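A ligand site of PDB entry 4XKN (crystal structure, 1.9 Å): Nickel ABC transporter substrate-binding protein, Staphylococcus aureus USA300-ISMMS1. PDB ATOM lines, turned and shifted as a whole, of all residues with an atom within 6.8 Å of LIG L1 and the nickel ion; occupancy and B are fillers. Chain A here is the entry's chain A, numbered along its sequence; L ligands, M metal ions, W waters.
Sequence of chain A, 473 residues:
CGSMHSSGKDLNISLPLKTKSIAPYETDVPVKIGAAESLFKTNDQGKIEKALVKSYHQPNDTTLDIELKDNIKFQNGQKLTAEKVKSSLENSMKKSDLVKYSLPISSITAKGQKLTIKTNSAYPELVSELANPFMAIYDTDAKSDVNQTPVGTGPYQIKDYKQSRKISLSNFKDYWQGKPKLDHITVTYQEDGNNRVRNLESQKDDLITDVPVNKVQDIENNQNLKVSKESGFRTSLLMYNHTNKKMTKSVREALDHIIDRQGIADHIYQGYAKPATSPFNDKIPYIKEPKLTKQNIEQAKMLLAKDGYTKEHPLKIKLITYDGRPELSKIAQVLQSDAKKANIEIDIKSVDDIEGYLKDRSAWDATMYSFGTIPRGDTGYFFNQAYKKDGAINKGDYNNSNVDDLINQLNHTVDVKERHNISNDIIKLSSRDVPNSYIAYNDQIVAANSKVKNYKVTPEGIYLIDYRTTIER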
ATOM      1  N   PRO A  16     -22.973  -3.545  25.398  1.00  0.00           N
ATOM      2  CA  PRO A  16     -22.184  -4.559  26.104  1.00  0.00           C
ATOM      3  C   PRO A  16     -20.684  -4.289  25.904  1.00  0.00           C
ATOM      4  O   PRO A  16     -20.352  -3.401  25.129  1.00  0.00           O
ATOM      5  CB  PRO A  16     -22.584  -5.860  25.412  1.00  0.00           C
ATOM      6  CG  PRO A  16     -22.801  -5.447  23.988  1.00  0.00           C
ATOM      7  CD  PRO A  16     -23.390  -4.023  24.061  1.00  0.00           C
ATOM      8  N   LEU A  17     -19.828  -5.062  26.582  1.00  0.00           N
ATOM      9  CA  LEU A  17     -18.373  -5.125  26.349  1.00  0.00           C
ATOM     10  C   LEU A  17     -17.671  -3.848  26.768  1.00  0.00           C
ATOM     11  O   LEU A  17     -17.075  -3.106  25.955  1.00  0.00           O
ATOM     12  CB  LEU A  17     -18.069  -5.449  24.874  1.00  0.00           C
ATOM     13  CG  LEU A  17     -18.744  -6.730  24.340  1.00  0.00           C
ATOM     14  CD1 LEU A  17     -18.265  -7.024  22.911  1.00  0.00           C
ATOM     15  CD2 LEU A  17     -18.519  -7.917  25.264  1.00  0.00           C
ATOM     16  N   LYS A  18     -17.720  -3.597  28.069  1.00  0.00           N
ATOM     17  CA  LYS A  18     -17.097  -2.405  28.645  1.00  0.00           C
ATOM     18  C   LYS A  18     -15.619  -2.330  28.280  1.00  0.00           C
ATOM     19  O   LYS A  18     -14.919  -3.334  28.181  1.00  0.00           O
ATOM     20  CB  LYS A  18     -17.257  -2.405  30.170  1.00  0.00           C
ATOM     21  CG  LYS A  18     -16.688  -3.621  30.850  1.00  0.00           C
ATOM     22  CD  LYS A  18     -17.212  -3.733  32.281  1.00  0.00           C
ATOM     23  CE  LYS A  18     -16.068  -3.930  33.233  1.00  0.00           C
ATOM     24  NZ  LYS A  18     -16.541  -3.983  34.643  1.00  0.00           N
ATOM     25  N   THR A  19     -15.175  -1.101  28.087  1.00  0.00           N
ATOM     26  CA  THR A  19     -13.816  -0.813  27.708  1.00  0.00           C
ATOM     27  C   THR A  19     -12.990  -0.382  28.908  1.00  0.00           C
ATOM     28  O   THR A  19     -13.537  -0.044  29.954  1.00  0.00           O
ATOM     29  CB  THR A  19     -13.778   0.315  26.673  1.00  0.00           C
ATOM     30  OG1 THR A  19     -14.635   1.371  27.141  1.00  0.00           O
ATOM     31  CG2 THR A  19     -14.268  -0.184  25.319  1.00  0.00           C
ATOM     32  N   THR A  27     -10.077   0.063  20.775  1.00  0.00           N
ATOM     33  CA  THR A  27     -11.468  -0.362  20.686  1.00  0.00           C
ATOM     34  C   THR A  27     -12.156   0.328  19.518  1.00  0.00           C
ATOM     35  O   THR A  27     -11.771   1.439  19.139  1.00  0.00           O
ATOM     36  CB  THR A  27     -12.241  -0.050  21.991  1.00  0.00           C
ATOM     37  OG1 THR A  27     -13.640  -0.212  21.761  1.00  0.00           O
ATOM     38  CG2 THR A  27     -11.946   1.382  22.476  1.00  0.00           C
ATOM     39  N   ASP A  28     -13.162  -0.313  18.931  1.00  0.00           N
ATOM     40  CA  ASP A  28     -13.885   0.323  17.831  1.00  0.00           C
ATOM     41  C   ASP A  28     -15.034   1.186  18.360  1.00  0.00           C
ATOM     42  O   ASP A  28     -15.781   1.783  17.596  1.00  0.00           O
ATOM     43  CB  ASP A  28     -14.375  -0.722  16.818  1.00  0.00           C
ATOM     44  CG  ASP A  28     -15.389  -1.720  17.399  1.00  0.00           C
ATOM     45  OD1 ASP A  28     -15.897  -1.529  18.516  1.00  0.00           O
ATOM     46  OD2 ASP A  28     -15.696  -2.708  16.689  1.00  0.00           O
ATOM     47  N   PHE A 134     -10.094   0.536  14.121  1.00  0.00           N
ATOM     48  CA  PHE A 134      -8.950   0.669  15.013  1.00  0.00           C
ATOM     49  C   PHE A 134      -7.922   1.638  14.405  1.00  0.00           C
ATOM     50  O   PHE A 134      -7.002   2.099  15.102  1.00  0.00           O
ATOM     51  CB  PHE A 134      -8.309  -0.692  15.321  1.00  0.00           C
ATOM     52  CG  PHE A 134      -9.050  -1.486  16.350  1.00  0.00           C
ATOM     53  CD1 PHE A 134     -10.296  -2.010  16.065  1.00  0.00           C
ATOM     54  CD2 PHE A 134      -8.515  -1.690  17.625  1.00  0.00           C
ATOM     55  CE1 PHE A 134     -10.995  -2.735  17.007  1.00  0.00           C
ATOM     56  CE2 PHE A 134      -9.209  -2.407  18.564  1.00  0.00           C
ATOM     57  CZ  PHE A 134     -10.449  -2.930  18.255  1.00  0.00           C
ATOM     58  N   ARG A 234     -20.724 -11.688  11.879  1.00  0.00           N
ATOM     59  CA  ARG A 234     -20.180 -12.055  13.189  1.00  0.00           C
ATOM     60  C   ARG A 234     -20.357 -13.578  13.378  1.00  0.00           C
ATOM     61  O   ARG A 234     -21.386 -14.158  13.020  1.00  0.00           O
ATOM     62  CB  ARG A 234     -20.884 -11.260  14.318  1.00  0.00           C
ATOM     63  CG  ARG A 234     -20.530 -11.707  15.741  1.00  0.00           C
ATOM     64  CD  ARG A 234     -20.796 -10.584  16.754  1.00  0.00           C
ATOM     65  NE  ARG A 234     -20.008  -9.425  16.412  1.00  0.00           N
ATOM     66  CZ  ARG A 234     -18.750  -9.229  16.791  1.00  0.00           C
ATOM     67  NH1 ARG A 234     -18.140 -10.092  17.596  1.00  0.00           N
ATOM     68  NH2 ARG A 234     -18.109  -8.147  16.385  1.00  0.00           N
ATOM     69  N   TYR A 322     -18.756 -15.008  28.819  1.00  0.00           N
ATOM     70  CA  TYR A 322     -19.053 -13.619  29.189  1.00  0.00           C
ATOM     71  C   TYR A 322     -20.464 -13.291  28.688  1.00  0.00           C
ATOM     72  O   TYR A 322     -20.956 -13.956  27.768  1.00  0.00           O
ATOM     73  CB  TYR A 322     -17.999 -12.628  28.623  1.00  0.00           C
ATOM     74  CG  TYR A 322     -17.777 -12.663  27.106  1.00  0.00           C
ATOM     75  CD1 TYR A 322     -17.015 -13.677  26.510  1.00  0.00           C
ATOM     76  CD2 TYR A 322     -18.297 -11.667  26.279  1.00  0.00           C
ATOM     77  CE1 TYR A 322     -16.789 -13.699  25.122  1.00  0.00           C
ATOM     78  CE2 TYR A 322     -18.075 -11.684  24.899  1.00  0.00           C
ATOM     79  CZ  TYR A 322     -17.332 -12.705  24.323  1.00  0.00           C
ATOM     80  OH  TYR A 322     -17.120 -12.725  22.953  1.00  0.00           O
ATOM     81  N   GLY A 324     -21.809 -10.308  27.384  1.00  0.00           N
ATOM     82  CA  GLY A 324     -22.015  -9.300  26.348  1.00  0.00           C
ATOM     83  C   GLY A 324     -22.754  -9.785  25.103  1.00  0.00           C
ATOM     84  O   GLY A 324     -23.669  -9.123  24.613  1.00  0.00           O
ATOM     85  N   ARG A 325     -22.330 -10.935  24.583  1.00  0.00           N
ATOM     86  CA  ARG A 325     -23.062 -11.598  23.516  1.00  0.00           C
ATOM     87  C   ARG A 325     -23.955 -12.620  24.215  1.00  0.00           C
ATOM     88  O   ARG A 325     -23.478 -13.645  24.710  1.00  0.00           O
ATOM     89  CB  ARG A 325     -22.099 -12.267  22.514  1.00  0.00           C
ATOM     90  CG  ARG A 325     -20.891 -11.416  22.109  1.00  0.00           C
ATOM     91  CD  ARG A 325     -21.279 -10.290  21.099  1.00  0.00           C
ATOM     92  NE  ARG A 325     -20.094  -9.534  20.650  1.00  0.00           N
ATOM     93  CZ  ARG A 325     -20.138  -8.370  20.001  1.00  0.00           C
ATOM     94  NH1 ARG A 325     -21.295  -7.817  19.706  1.00  0.00           N
ATOM     95  NH2 ARG A 325     -19.024  -7.753  19.629  1.00  0.00           N
ATOM     96  N   LEU A 328     -23.843 -16.688  24.107  1.00  0.00           N
ATOM     97  CA  LEU A 328     -22.609 -17.419  24.365  1.00  0.00           C
ATOM     98  C   LEU A 328     -22.718 -18.299  25.635  1.00  0.00           C
ATOM     99  O   LEU A 328     -22.330 -19.452  25.622  1.00  0.00           O
ATOM    100  CB  LEU A 328     -21.406 -16.460  24.493  1.00  0.00           C
ATOM    101  CG  LEU A 328     -20.885 -15.827  23.180  1.00  0.00           C
ATOM    102  CD1 LEU A 328     -19.644 -15.024  23.423  1.00  0.00           C
ATOM    103  CD2 LEU A 328     -20.618 -16.851  22.061  1.00  0.00           C
ATOM    104  N   ASP A 353     -14.535  -8.988  32.092  1.00  0.00           N
ATOM    105  CA  ASP A 353     -13.608  -8.365  31.142  1.00  0.00           C
ATOM    106  C   ASP A 353     -12.923  -9.451  30.319  1.00  0.00           C
ATOM    107  O   ASP A 353     -11.827  -9.899  30.681  1.00  0.00           O
ATOM    108  CB  ASP A 353     -12.584  -7.511  31.907  1.00  0.00           C
ATOM    109  CG  ASP A 353     -11.475  -6.941  31.024  1.00  0.00           C
ATOM    110  OD1 ASP A 353     -11.627  -6.921  29.782  1.00  0.00           O
ATOM    111  OD2 ASP A 353     -10.453  -6.511  31.587  1.00  0.00           O
ATOM    112  N   ILE A 354     -13.553  -9.899  29.250  1.00  0.00           N
ATOM    113  CA  ILE A 354     -13.044 -11.084  28.549  1.00  0.00           C
ATOM    114  C   ILE A 354     -11.655 -10.843  27.923  1.00  0.00           C
ATOM    115  O   ILE A 354     -10.779 -11.702  28.009  1.00  0.00           O
ATOM    116  CB  ILE A 354     -14.059 -11.582  27.468  1.00  0.00           C
ATOM    117  CG1 ILE A 354     -13.571 -12.886  26.807  1.00  0.00           C
ATOM    118  CG2 ILE A 354     -14.363 -10.486  26.408  1.00  0.00           C
ATOM    119  CD1 ILE A 354     -13.480 -14.070  27.796  1.00  0.00           C
ATOM    120  N   GLU A 355     -11.431  -9.685  27.305  1.00  0.00           N
ATOM    121  CA  GLU A 355     -10.160  -9.423  26.634  1.00  0.00           C
ATOM    122  C   GLU A 355      -9.007  -9.416  27.642  1.00  0.00           C
ATOM    123  O   GLU A 355      -7.942  -9.962  27.390  1.00  0.00           O
ATOM    124  CB  GLU A 355     -10.209  -8.101  25.861  1.00  0.00           C
ATOM    125  CG  GLU A 355     -11.205  -8.125  24.675  1.00  0.00           C
ATOM    126  CD  GLU A 355     -10.770  -9.087  23.575  1.00  0.00           C
ATOM    127  OE1 GLU A 355      -9.926  -8.706  22.738  1.00  0.00           O
ATOM    128  OE2 GLU A 355     -11.249 -10.260  23.574  1.00  0.00           O
ATOM    129  N   TYR A 369     -16.335 -17.302  22.383  1.00  0.00           N
ATOM    130  CA  TYR A 369     -15.847 -16.072  21.769  1.00  0.00           C
ATOM    131  C   TYR A 369     -16.729 -15.689  20.595  1.00  0.00           C
ATOM    132  O   TYR A 369     -17.546 -16.472  20.111  1.00  0.00           O
ATOM    133  CB  TYR A 369     -14.377 -16.222  21.321  1.00  0.00           C
ATOM    134  CG  TYR A 369     -13.602 -14.925  21.324  1.00  0.00           C
ATOM    135  CD1 TYR A 369     -13.266 -14.286  22.517  1.00  0.00           C
ATOM    136  CD2 TYR A 369     -13.203 -14.328  20.125  1.00  0.00           C
ATOM    137  CE1 TYR A 369     -12.548 -13.090  22.514  1.00  0.00           C
ATOM    138  CE2 TYR A 369     -12.496 -13.138  20.118  1.00  0.00           C
ATOM    139  CZ  TYR A 369     -12.162 -12.526  21.302  1.00  0.00           C
ATOM    140  OH  TYR A 369     -11.477 -11.328  21.276  1.00  0.00           O
ATOM    141  N   SER A 370     -16.581 -14.453  20.163  1.00  0.00           N
ATOM    142  CA  SER A 370     -17.361 -13.911  19.078  1.00  0.00           C
ATOM    143  C   SER A 370     -16.498 -12.879  18.354  1.00  0.00           C
ATOM    144  O   SER A 370     -15.868 -12.057  18.996  1.00  0.00           O
ATOM    145  CB  SER A 370     -18.636 -13.249  19.611  1.00  0.00           C
ATOM    146  OG  SER A 370     -19.356 -12.640  18.546  1.00  0.00           O
ATOM    147  N   PHE A 371     -16.470 -12.918  17.034  1.00  0.00           N
ATOM    148  CA  PHE A 371     -15.637 -11.963  16.315  1.00  0.00           C
ATOM    149  C   PHE A 371     -16.239 -11.599  14.961  1.00  0.00           C
ATOM    150  O   PHE A 371     -16.934 -12.408  14.352  1.00  0.00           O
ATOM    151  CB  PHE A 371     -14.222 -12.533  16.117  1.00  0.00           C
ATOM    152  CG  PHE A 371     -13.223 -11.527  15.575  1.00  0.00           C
ATOM    153  CD1 PHE A 371     -12.878 -10.404  16.325  1.00  0.00           C
ATOM    154  CD2 PHE A 371     -12.644 -11.703  14.331  1.00  0.00           C
ATOM    155  CE1 PHE A 371     -11.969  -9.482  15.840  1.00  0.00           C
ATOM    156  CE2 PHE A 371     -11.733 -10.776  13.829  1.00  0.00           C
ATOM    157  CZ  PHE A 371     -11.398  -9.670  14.584  1.00  0.00           C
ATOM    158  N   GLY A 372     -15.973 -10.384  14.492  1.00  0.00           N
ATOM    159  CA  GLY A 372     -16.393  -9.976  13.164  1.00  0.00           C
ATOM    160  C   GLY A 372     -15.322 -10.468  12.203  1.00  0.00           C
ATOM    161  O   GLY A 372     -14.286  -9.823  12.048  1.00  0.00           O
ATOM    162  N   ILE A 393      -6.263 -11.301  17.964  1.00  0.00           N
ATOM    163  CA  ILE A 393      -7.317 -12.111  18.570  1.00  0.00           C
ATOM    164  C   ILE A 393      -6.954 -13.593  18.615  1.00  0.00           C
ATOM    165  O   ILE A 393      -7.809 -14.434  18.877  1.00  0.00           O
ATOM    166  CB  ILE A 393      -8.679 -11.939  17.853  1.00  0.00           C
ATOM    167  CG1 ILE A 393      -8.636 -12.473  16.443  1.00  0.00           C
ATOM    168  CG2 ILE A 393      -9.163 -10.468  17.931  1.00  0.00           C
ATOM    169  CD1 ILE A 393      -9.973 -13.037  16.008  1.00  0.00           C
ATOM    170  N   LYS A 395      -5.978 -15.507  20.825  1.00  0.00           N
ATOM    171  CA  LYS A 395      -5.850 -15.614  22.286  1.00  0.00           C
ATOM    172  C   LYS A 395      -5.212 -16.947  22.722  1.00  0.00           C
ATOM    173  O   LYS A 395      -4.521 -16.996  23.744  1.00  0.00           O
ATOM    174  CB  LYS A 395      -7.214 -15.465  22.976  1.00  0.00           C
ATOM    175  CG  LYS A 395      -8.093 -14.307  22.483  1.00  0.00           C
ATOM    176  CD  LYS A 395      -7.385 -12.939  22.546  1.00  0.00           C
ATOM    177  CE  LYS A 395      -8.384 -11.824  22.307  1.00  0.00           C
ATOM    178  NZ  LYS A 395      -7.756 -10.451  22.387  1.00  0.00           N
HETATM  179  N1  LIG L   1     -14.194 -10.087  20.499  1.00  0.00           N
HETATM  180  C1  LIG L   1     -15.172 -10.433  21.541  1.00  0.00           C
HETATM  181  C2  LIG L   1     -16.547  -9.898  21.194  1.00  0.00           C
HETATM  182  O1  LIG L   1     -16.638  -8.892  20.487  1.00  0.00           O
HETATM  183  C3  LIG L   1     -14.726  -9.888  22.919  1.00  0.00           C
HETATM  184  C4  LIG L   1     -14.648  -8.391  22.998  1.00  0.00           C
HETATM  185  N2  LIG L   1     -14.503  -7.575  21.901  1.00  0.00           N
HETATM  186  C5  LIG L   1     -14.686  -7.554  24.073  1.00  0.00           C
HETATM  187  C6  LIG L   1     -14.461  -6.314  22.279  1.00  0.00           C
HETATM  188  N3  LIG L   1     -14.584  -6.278  23.599  1.00  0.00           N
HETATM  189  O2  LIG L   1     -17.576 -10.454  21.617  1.00  0.00           O
HETATM  190  N1  LG2 L   2     -15.370  -6.246  19.098  1.00  0.00           N
HETATM  191  C1  LG2 L   2     -14.974  -6.341  17.687  1.00  0.00           C
HETATM  192  C2  LG2 L   2     -15.130  -7.772  17.165  1.00  0.00           C
HETATM  193  O1  LG2 L   2     -15.160  -7.987  15.940  1.00  0.00           O
HETATM  194  C3  LG2 L   2     -13.520  -5.851  17.486  1.00  0.00           C
HETATM  195  C4  LG2 L   2     -12.489  -6.566  18.300  1.00  0.00           C
HETATM  196  N2  LG2 L   2     -12.808  -7.507  19.280  1.00  0.00           N
HETATM  197  C5  LG2 L   2     -11.136  -6.494  18.306  1.00  0.00           C
HETATM  198  C6  LG2 L   2     -11.709  -7.954  19.846  1.00  0.00           C
HETATM  199  N3  LG2 L   2     -10.670  -7.356  19.267  1.00  0.00           N
HETATM  200  O2  LG2 L   2     -15.223  -8.746  17.927  1.00  0.00           O
HETATM  201 NI    NI M   1     -14.715  -8.120  19.923  1.00  0.00          NI
HETATM  202  O   HOH W   1     -14.504  -3.785  24.914  1.00  0.00           O
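No residue comes within 4 Å of the nickel ion. The nearest printed residue that does not touch the nickel ion is Ser 370 (4.2 Å).
N of Ser 370 is in hydrogen-bond range of OH of Tyr 322 (3.3 Å). The guanidinium group (NH1) of Arg 234 is in hydrogen-bond range of the side-chain hydroxyl (OG) of Ser 370 (3.0 Å). The side-chain hydroxyl of Tyr 369 lies within hydrogen-bond range of the side-chain carboxylate of Glu 355. NZ of Lys 395 lies within salt-bridge range of OE1 of Glu 355 (2.8 Å).
Water W1 lies within hydrogen-bond range of N3 of LIG L1 (2.8 Å), O of Leu 17 (2.9 Å) and O of Lys 18 (3.3 Å).
The nickel ion is bound by a nitrogen (N2) of LIG L1 (2.1 Å), a nitrogen (N2) of LG2 L2 (2.1 Å), a nitrogen (N1) of LIG L1 (2.1 Å), an oxygen (O1) of LIG L1 (2.1 Å), a nitrogen (N1) of LG2 L2 (2.1 Å) and an oxygen (O2) of LG2 L2 (2.2 Å). The nickel ion has six donor atoms within binding distance.
Residues that only touch LIG L1: Leu 17, Glu 355 and Ile 354. Hydrophobic or aromatic side chains within 4 Å of LIG L1: Leu 17, Tyr 322, Ile 354 and Tyr 369. Within 4 Å of LIG L1: Leu 17, Arg 234, Tyr 322, Arg 325, Ile 354, Glu 355, Tyr 369 and Ser 370. The nearest printed residue that does not touch LIG L1 is Phe 371 (4.4 Å).
The side-chain hydroxyl of Tyr 322 is in hydrogen-bond range of an oxygen (O2) of LIG L1, at 2.7 Å. An oxygen (O2) of LIG L1 is in salt-bridge range of the guanidinium group of Arg 325 (2.8 Å). The backbone carbonyl oxygen (O) of Ser 370 sits close to a nitrogen (N1) of LIG L1, at 3.0 Å. N1 of LIG L1 lies close to OH of Tyr 369, 3.1 Å away. O1 of LIG L1 lies close to NH1 of Arg 234. An oxygen (O1) of LG2 L2 is in salt-bridge range of the guanidinium group (NH2) of Arg 234 (3.0 Å). O1 of LG2 L2 lies within hydrogen-bond range of N of Gly 372.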
